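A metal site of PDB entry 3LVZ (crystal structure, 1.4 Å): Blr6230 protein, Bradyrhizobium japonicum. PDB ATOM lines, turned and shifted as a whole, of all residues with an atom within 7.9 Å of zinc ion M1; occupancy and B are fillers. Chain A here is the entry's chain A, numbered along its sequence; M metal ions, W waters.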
ATOM      1  N   PHE A  26     -34.025   9.281 -15.184  1.00  0.00           N
ATOM      2  CA  PHE A  26     -33.689   9.499 -16.572  1.00  0.00           C
ATOM      3  C   PHE A  26     -34.230   8.307 -17.471  1.00  0.00           C
ATOM      4  O   PHE A  26     -34.865   8.491 -18.531  1.00  0.00           O
ATOM      5  CB  PHE A  26     -32.156   9.647 -16.672  1.00  0.00           C
ATOM      6  CG  PHE A  26     -31.670   9.862 -18.094  1.00  0.00           C
ATOM      7  CD1 PHE A  26     -31.566  11.146 -18.615  1.00  0.00           C
ATOM      8  CD2 PHE A  26     -31.362   8.767 -18.901  1.00  0.00           C
ATOM      9  CE1 PHE A  26     -31.121  11.333 -19.925  1.00  0.00           C
ATOM     10  CE2 PHE A  26     -30.938   8.942 -20.197  1.00  0.00           C
ATOM     11  CZ  PHE A  26     -30.807  10.196 -20.703  1.00  0.00           C
ATOM     12  N   TRP A  34     -40.508   9.879 -23.787  1.00  0.00           N
ATOM     13  CA  TRP A  34     -39.521   9.848 -24.861  1.00  0.00           C
ATOM     14  C   TRP A  34     -39.811   8.829 -25.899  1.00  0.00           C
ATOM     15  O   TRP A  34     -39.309   8.959 -27.033  1.00  0.00           O
ATOM     16  CB  TRP A  34     -38.118   9.598 -24.334  1.00  0.00           C
ATOM     17  CG  TRP A  34     -37.498  10.741 -23.625  1.00  0.00           C
ATOM     18  CD1 TRP A  34     -38.064  11.965 -23.299  1.00  0.00           C
ATOM     19  CD2 TRP A  34     -36.145  10.822 -23.167  1.00  0.00           C
ATOM     20  NE1 TRP A  34     -37.167  12.754 -22.683  1.00  0.00           N
ATOM     21  CE2 TRP A  34     -35.966  12.100 -22.602  1.00  0.00           C
ATOM     22  CE3 TRP A  34     -35.091   9.914 -23.145  1.00  0.00           C
ATOM     23  CZ2 TRP A  34     -34.755  12.514 -22.039  1.00  0.00           C
ATOM     24  CZ3 TRP A  34     -33.879  10.357 -22.527  1.00  0.00           C
ATOM     25  CH2 TRP A  34     -33.752  11.630 -22.060  1.00  0.00           C
ATOM     26  N   THR A 100     -26.841  17.138 -32.978  1.00  0.00           N
ATOM     27  CA  THR A 100     -26.777  18.234 -32.013  1.00  0.00           C
ATOM     28  C   THR A 100     -25.748  17.851 -30.919  1.00  0.00           C
ATOM     29  O   THR A 100     -24.794  18.565 -30.646  1.00  0.00           O
ATOM     30  CB  THR A 100     -28.111  18.545 -31.337  1.00  0.00           C
ATOM     31  OG1 THR A 100     -28.722  17.365 -30.844  1.00  0.00           O
ATOM     32  CG2 THR A 100     -28.973  19.348 -32.229  1.00  0.00           C
ATOM     33  N   HIS A 101     -25.932  16.744 -30.238  1.00  0.00           N
ATOM     34  CA  HIS A 101     -24.991  16.271 -29.267  1.00  0.00           C
ATOM     35  C   HIS A 101     -25.039  14.787 -29.017  1.00  0.00           C
ATOM     36  O   HIS A 101     -26.097  14.163 -29.268  1.00  0.00           O
ATOM     37  CB  HIS A 101     -25.145  17.020 -27.941  1.00  0.00           C
ATOM     38  CG  HIS A 101     -26.315  16.643 -27.082  1.00  0.00           C
ATOM     39  ND1 HIS A 101     -27.518  17.232 -27.220  1.00  0.00           N
ATOM     40  CD2 HIS A 101     -26.476  15.679 -26.145  1.00  0.00           C
ATOM     41  CE1 HIS A 101     -28.345  16.695 -26.326  1.00  0.00           C
ATOM     42  NE2 HIS A 101     -27.761  15.719 -25.685  1.00  0.00           N
ATOM     43  N   ALA A 102     -23.929  14.228 -28.528  1.00  0.00           N
ATOM     44  CA  ALA A 102     -23.745  12.796 -28.576  1.00  0.00           C
ATOM     45  C   ALA A 102     -24.175  12.065 -27.348  1.00  0.00           C
ATOM     46  O   ALA A 102     -23.337  11.452 -26.705  1.00  0.00           O
ATOM     47  CB  ALA A 102     -22.265  12.486 -28.924  1.00  0.00           C
ATOM     48  N   HIS A 103     -25.457  12.123 -26.979  1.00  0.00           N
ATOM     49  CA  HIS A 103     -26.054  11.282 -25.937  1.00  0.00           C
ATOM     50  C   HIS A 103     -27.033  10.298 -26.549  1.00  0.00           C
ATOM     51  O   HIS A 103     -27.620  10.619 -27.617  1.00  0.00           O
ATOM     52  CB  HIS A 103     -26.791  12.121 -24.920  1.00  0.00           C
ATOM     53  CG  HIS A 103     -25.943  12.982 -24.062  1.00  0.00           C
ATOM     54  ND1 HIS A 103     -26.431  14.104 -23.413  1.00  0.00           N
ATOM     55  CD2 HIS A 103     -24.653  12.825 -23.690  1.00  0.00           C
ATOM     56  CE1 HIS A 103     -25.446  14.591 -22.674  1.00  0.00           C
ATOM     57  NE2 HIS A 103     -24.345  13.875 -22.853  1.00  0.00           N
ATOM     58  N   LEU A 104     -27.269   9.142 -25.916  1.00  0.00           N
ATOM     59  CA  LEU A 104     -28.021   8.044 -26.500  1.00  0.00           C
ATOM     60  C   LEU A 104     -29.419   8.402 -26.913  1.00  0.00           C
ATOM     61  O   LEU A 104     -29.968   7.787 -27.819  1.00  0.00           O
ATOM     62  CB  LEU A 104     -28.070   6.851 -25.594  1.00  0.00           C
ATOM     63  CG  LEU A 104     -29.061   6.799 -24.486  1.00  0.00           C
ATOM     64  CD1 LEU A 104     -29.159   5.374 -24.005  1.00  0.00           C
ATOM     65  CD2 LEU A 104     -28.687   7.715 -23.342  1.00  0.00           C
ATOM     66  N   ASP A 105     -30.037   9.392 -26.278  1.00  0.00           N
ATOM     67  CA  ASP A 105     -31.422   9.737 -26.668  1.00  0.00           C
ATOM     68  C   ASP A 105     -31.506  10.514 -27.974  1.00  0.00           C
ATOM     69  O   ASP A 105     -32.601  10.748 -28.496  1.00  0.00           O
ATOM     70  CB  ASP A 105     -32.126  10.514 -25.502  1.00  0.00           C
ATOM     71  CG  ASP A 105     -31.408  11.692 -24.984  1.00  0.00           C
ATOM     72  OD1 ASP A 105     -30.141  11.705 -24.822  1.00  0.00           O
ATOM     73  OD2 ASP A 105     -32.106  12.745 -24.705  1.00  0.00           O
ATOM     74  N   HIS A 106     -30.348  10.874 -28.516  1.00  0.00           N
ATOM     75  CA  HIS A 106     -30.213  11.578 -29.812  1.00  0.00           C
ATOM     76  C   HIS A 106     -29.415  10.801 -30.840  1.00  0.00           C
ATOM     77  O   HIS A 106     -29.572  11.054 -32.031  1.00  0.00           O
ATOM     78  CB  HIS A 106     -29.674  12.980 -29.674  1.00  0.00           C
ATOM     79  CG  HIS A 106     -30.372  13.740 -28.611  1.00  0.00           C
ATOM     80  ND1 HIS A 106     -31.706  14.092 -28.739  1.00  0.00           N
ATOM     81  CD2 HIS A 106     -30.014  14.039 -27.334  1.00  0.00           C
ATOM     82  CE1 HIS A 106     -32.106  14.645 -27.596  1.00  0.00           C
ATOM     83  NE2 HIS A 106     -31.082  14.633 -26.722  1.00  0.00           N
ATOM     84  N   TYR A 136     -21.282   7.451 -22.513  1.00  0.00           N
ATOM     85  CA  TYR A 136     -21.550   8.728 -21.825  1.00  0.00           C
ATOM     86  C   TYR A 136     -20.260   9.247 -21.182  1.00  0.00           C
ATOM     87  O   TYR A 136     -19.659   8.528 -20.422  1.00  0.00           O
ATOM     88  CB  TYR A 136     -22.652   8.578 -20.754  1.00  0.00           C
ATOM     89  CG  TYR A 136     -23.245   9.875 -20.336  1.00  0.00           C
ATOM     90  CD1 TYR A 136     -24.408  10.323 -20.899  1.00  0.00           C
ATOM     91  CD2 TYR A 136     -22.616  10.698 -19.413  1.00  0.00           C
ATOM     92  CE1 TYR A 136     -24.935  11.548 -20.583  1.00  0.00           C
ATOM     93  CE2 TYR A 136     -23.123  11.944 -19.121  1.00  0.00           C
ATOM     94  CZ  TYR A 136     -24.263  12.382 -19.700  1.00  0.00           C
ATOM     95  OH  TYR A 136     -24.793  13.672 -19.432  1.00  0.00           O
ATOM     96  N   HIS A 177     -23.461  20.982 -22.359  1.00  0.00           N
ATOM     97  CA  HIS A 177     -24.262  19.737 -22.190  1.00  0.00           C
ATOM     98  C   HIS A 177     -23.504  18.536 -22.703  1.00  0.00           C
ATOM     99  O   HIS A 177     -23.614  17.431 -22.148  1.00  0.00           O
ATOM    100  CB  HIS A 177     -25.601  19.921 -22.861  1.00  0.00           C
ATOM    101  CG  HIS A 177     -26.495  18.739 -22.649  1.00  0.00           C
ATOM    102  ND1 HIS A 177     -27.351  18.602 -21.596  1.00  0.00           N
ATOM    103  CD2 HIS A 177     -26.743  17.681 -23.462  1.00  0.00           C
ATOM    104  CE1 HIS A 177     -27.997  17.443 -21.712  1.00  0.00           C
ATOM    105  NE2 HIS A 177     -27.618  16.855 -22.832  1.00  0.00           N
ATOM    106  N   SER A 178     -22.682  18.714 -23.730  1.00  0.00           N
ATOM    107  CA  SER A 178     -21.720  17.736 -24.142  1.00  0.00           C
ATOM    108  C   SER A 178     -20.475  18.516 -24.587  1.00  0.00           C
ATOM    109  O   SER A 178     -20.589  19.733 -24.942  1.00  0.00           O
ATOM    110  CB  SER A 178     -22.212  16.815 -25.296  1.00  0.00           C
ATOM    111  OG  SER A 178     -22.230  17.500 -26.499  1.00  0.00           O
ATOM    112  N   CYS A 181     -21.209  19.681 -28.255  1.00  0.00           N
ATOM    113  CA  CYS A 181     -22.575  20.141 -28.549  1.00  0.00           C
ATOM    114  C   CYS A 181     -22.576  21.190 -29.665  1.00  0.00           C
ATOM    115  O   CYS A 181     -21.857  22.242 -29.519  1.00  0.00           O
ATOM    116  CB  CYS A 181     -23.197  20.591 -27.232  1.00  0.00           C
ATOM    117  SG  CYS A 181     -24.872  20.596 -26.918  1.00  0.00           S
ATOM    118  N   CYS A 201     -28.556  22.989 -29.381  1.00  0.00           N
ATOM    119  CA  CYS A 201     -28.084  21.676 -29.056  1.00  0.00           C
ATOM    120  C   CYS A 201     -28.470  21.050 -27.756  1.00  0.00           C
ATOM    121  O   CYS A 201     -28.323  19.871 -27.627  1.00  0.00           O
ATOM    122  CB  CYS A 201     -26.561  21.607 -29.259  1.00  0.00           C
ATOM    123  SG  CYS A 201     -25.646  22.290 -27.922  1.00  0.00           S
ATOM    124  N   SER A 202     -28.870  21.858 -26.840  1.00  0.00           N
ATOM    125  CA  SER A 202     -29.217  21.588 -25.429  1.00  0.00           C
ATOM    126  C   SER A 202     -28.258  22.313 -24.481  1.00  0.00           C
ATOM    127  O   SER A 202     -27.044  22.351 -24.755  1.00  0.00           O
ATOM    128  CB  SER A 202     -29.251  20.125 -25.028  1.00  0.00           C
ATOM    129  OG  SER A 202     -29.441  20.108 -23.628  1.00  0.00           O
ATOM    130  N   GLY A 203     -28.813  22.922 -23.476  1.00  0.00           N
ATOM    131  CA  GLY A 203     -28.039  23.562 -22.427  1.00  0.00           C
ATOM    132  C   GLY A 203     -28.455  23.166 -21.003  1.00  0.00           C
ATOM    133  O   GLY A 203     -28.169  23.904 -20.030  1.00  0.00           O
ATOM    134  N   THR A 204     -29.093  22.038 -20.813  1.00  0.00           N
ATOM    135  CA  THR A 204     -29.477  21.567 -19.531  1.00  0.00           C
ATOM    136  C   THR A 204     -28.343  20.922 -18.815  1.00  0.00           C
ATOM    137  O   THR A 204     -27.369  20.457 -19.441  1.00  0.00           O
ATOM    138  CB  THR A 204     -30.609  20.516 -19.628  1.00  0.00           C
ATOM    139  OG1 THR A 204     -30.122  19.441 -20.419  1.00  0.00           O
ATOM    140  CG2 THR A 204     -31.885  21.155 -20.319  1.00  0.00           C
ATOM    141  N   VAL A 205     -28.376  20.974 -17.504  1.00  0.00           N
ATOM    142  CA  VAL A 205     -27.366  20.198 -16.706  1.00  0.00           C
ATOM    143  C   VAL A 205     -27.584  18.700 -16.759  1.00  0.00           C
ATOM    144  O   VAL A 205     -26.623  17.951 -16.976  1.00  0.00           O
ATOM    145  CB  VAL A 205     -27.258  20.733 -15.247  1.00  0.00           C
ATOM    146  CG1 VAL A 205     -26.278  19.832 -14.446  1.00  0.00           C
ATOM    147  CG2 VAL A 205     -26.904  22.216 -15.284  1.00  0.00           C
ATOM    148  N   ALA A 206     -28.831  18.289 -16.575  1.00  0.00           N
ATOM    149  CA  ALA A 206     -29.245  16.907 -16.721  1.00  0.00           C
ATOM    150  C   ALA A 206     -28.334  16.023 -15.895  1.00  0.00           C
ATOM    151  O   ALA A 206     -28.202  16.224 -14.633  1.00  0.00           O
ATOM    152  CB  ALA A 206     -29.304  16.553 -18.247  1.00  0.00           C
ATOM    153  N   LEU A 207     -27.684  15.034 -16.471  1.00  0.00           N
ATOM    154  CA  LEU A 207     -26.899  14.056 -15.675  1.00  0.00           C
ATOM    155  C   LEU A 207     -25.475  14.484 -15.429  1.00  0.00           C
ATOM    156  O   LEU A 207     -24.677  13.796 -14.813  1.00  0.00           O
ATOM    157  CB  LEU A 207     -26.838  12.699 -16.443  1.00  0.00           C
ATOM    158  CG  LEU A 207     -28.200  12.054 -16.629  1.00  0.00           C
ATOM    159  CD1 LEU A 207     -27.963  10.714 -17.401  1.00  0.00           C
ATOM    160  CD2 LEU A 207     -28.965  11.846 -15.403  1.00  0.00           C
ATOM    161  N   ASN A 208     -25.060  15.656 -15.952  1.00  0.00           N
ATOM    162  CA  ASN A 208     -23.625  16.000 -15.959  1.00  0.00           C
ATOM    163  C   ASN A 208     -23.183  16.410 -14.548  1.00  0.00           C
ATOM    164  O   ASN A 208     -23.952  17.029 -13.795  1.00  0.00           O
ATOM    165  CB  ASN A 208     -23.373  17.187 -16.906  1.00  0.00           C
ATOM    166  CG  ASN A 208     -23.465  16.794 -18.360  1.00  0.00           C
ATOM    167  OD1 ASN A 208     -23.169  15.601 -18.681  1.00  0.00           O
ATOM    168  ND2 ASN A 208     -23.777  17.721 -19.256  1.00  0.00           N
ATOM    169  N   PRO A 241     -33.433  19.593 -29.256  1.00  0.00           N
ATOM    170  CA  PRO A 241     -33.497  18.129 -29.360  1.00  0.00           C
ATOM    171  C   PRO A 241     -34.570  17.447 -28.480  1.00  0.00           C
ATOM    172  O   PRO A 241     -34.783  16.219 -28.603  1.00  0.00           O
ATOM    173  CB  PRO A 241     -32.044  17.753 -29.006  1.00  0.00           C
ATOM    174  CG  PRO A 241     -31.472  18.865 -28.312  1.00  0.00           C
ATOM    175  CD  PRO A 241     -32.238  20.106 -28.533  1.00  0.00           C
ATOM    176  N   HIS A 242     -35.301  18.212 -27.684  1.00  0.00           N
ATOM    177  CA  HIS A 242     -36.512  17.817 -27.013  1.00  0.00           C
ATOM    178  C   HIS A 242     -37.535  18.869 -27.243  1.00  0.00           C
ATOM    179  O   HIS A 242     -37.236  20.069 -27.255  1.00  0.00           O
ATOM    180  CB  HIS A 242     -36.183  17.653 -25.491  1.00  0.00           C
ATOM    181  CG  HIS A 242     -35.204  16.553 -25.215  1.00  0.00           C
ATOM    182  ND1 HIS A 242     -35.581  15.216 -25.099  1.00  0.00           N
ATOM    183  CD2 HIS A 242     -33.876  16.613 -24.951  1.00  0.00           C
ATOM    184  CE1 HIS A 242     -34.491  14.495 -24.835  1.00  0.00           C
ATOM    185  NE2 HIS A 242     -33.454  15.308 -24.720  1.00  0.00           N
HETATM  186 ZN    ZN M   1     -28.197  15.137 -23.763  1.00  0.00          ZN
HETATM  187 ZN    ZN M   2     -31.489  14.708 -24.697  1.00  0.00          ZN
HETATM  188  O   HOH W   1     -29.833  14.104 -23.636  1.00  0.00           O
HETATM  189  O   HOH W   2     -30.802  17.071 -24.132  1.00  0.00           O
HETATM  190  O   HOH W   3     -29.862  14.483 -21.003  1.00  0.00           O
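SG of Cys 201 is disulfide-bonded to SG of Cys 181, at 2.1 Å. A ring nitrogen (ND1) of His 177 sits at hydrogen-bond distance from the side-chain hydroxyl (OG) of Ser 202 (3.3 Å). The side-chain amide nitrogen of Asn 208 lies within hydrogen-bond range of the backbone carbonyl oxygen of His 177, at 2.9 Å. NE2 of His 103 sits close to OH of Tyr 136 (3.5 Å). A ring nitrogen (ND1) of His 177 sits at hydrogen-bond distance from the backbone carbonyl oxygen of Thr 204 (2.8 Å). O of Cys 201 sits at hydrogen-bond distance from ND1 of His 101, at 2.8 Å.
Within 4 Å of zinc ion M1: His 101, His 103 and His 177. Along chain A the residues within 4 Å of zinc ion M1 span positions 101 to 177.
Water W1 binds zinc ion M1 (1.9 Å). Zinc ion M1 is bound by a ring nitrogen (NE2) of His 177 (2.0 Å). NE2 of His 101 binds zinc ion M1 (2.1 Å). ND1 of His 103 is bound to zinc ion M1, at 2.1 Å.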
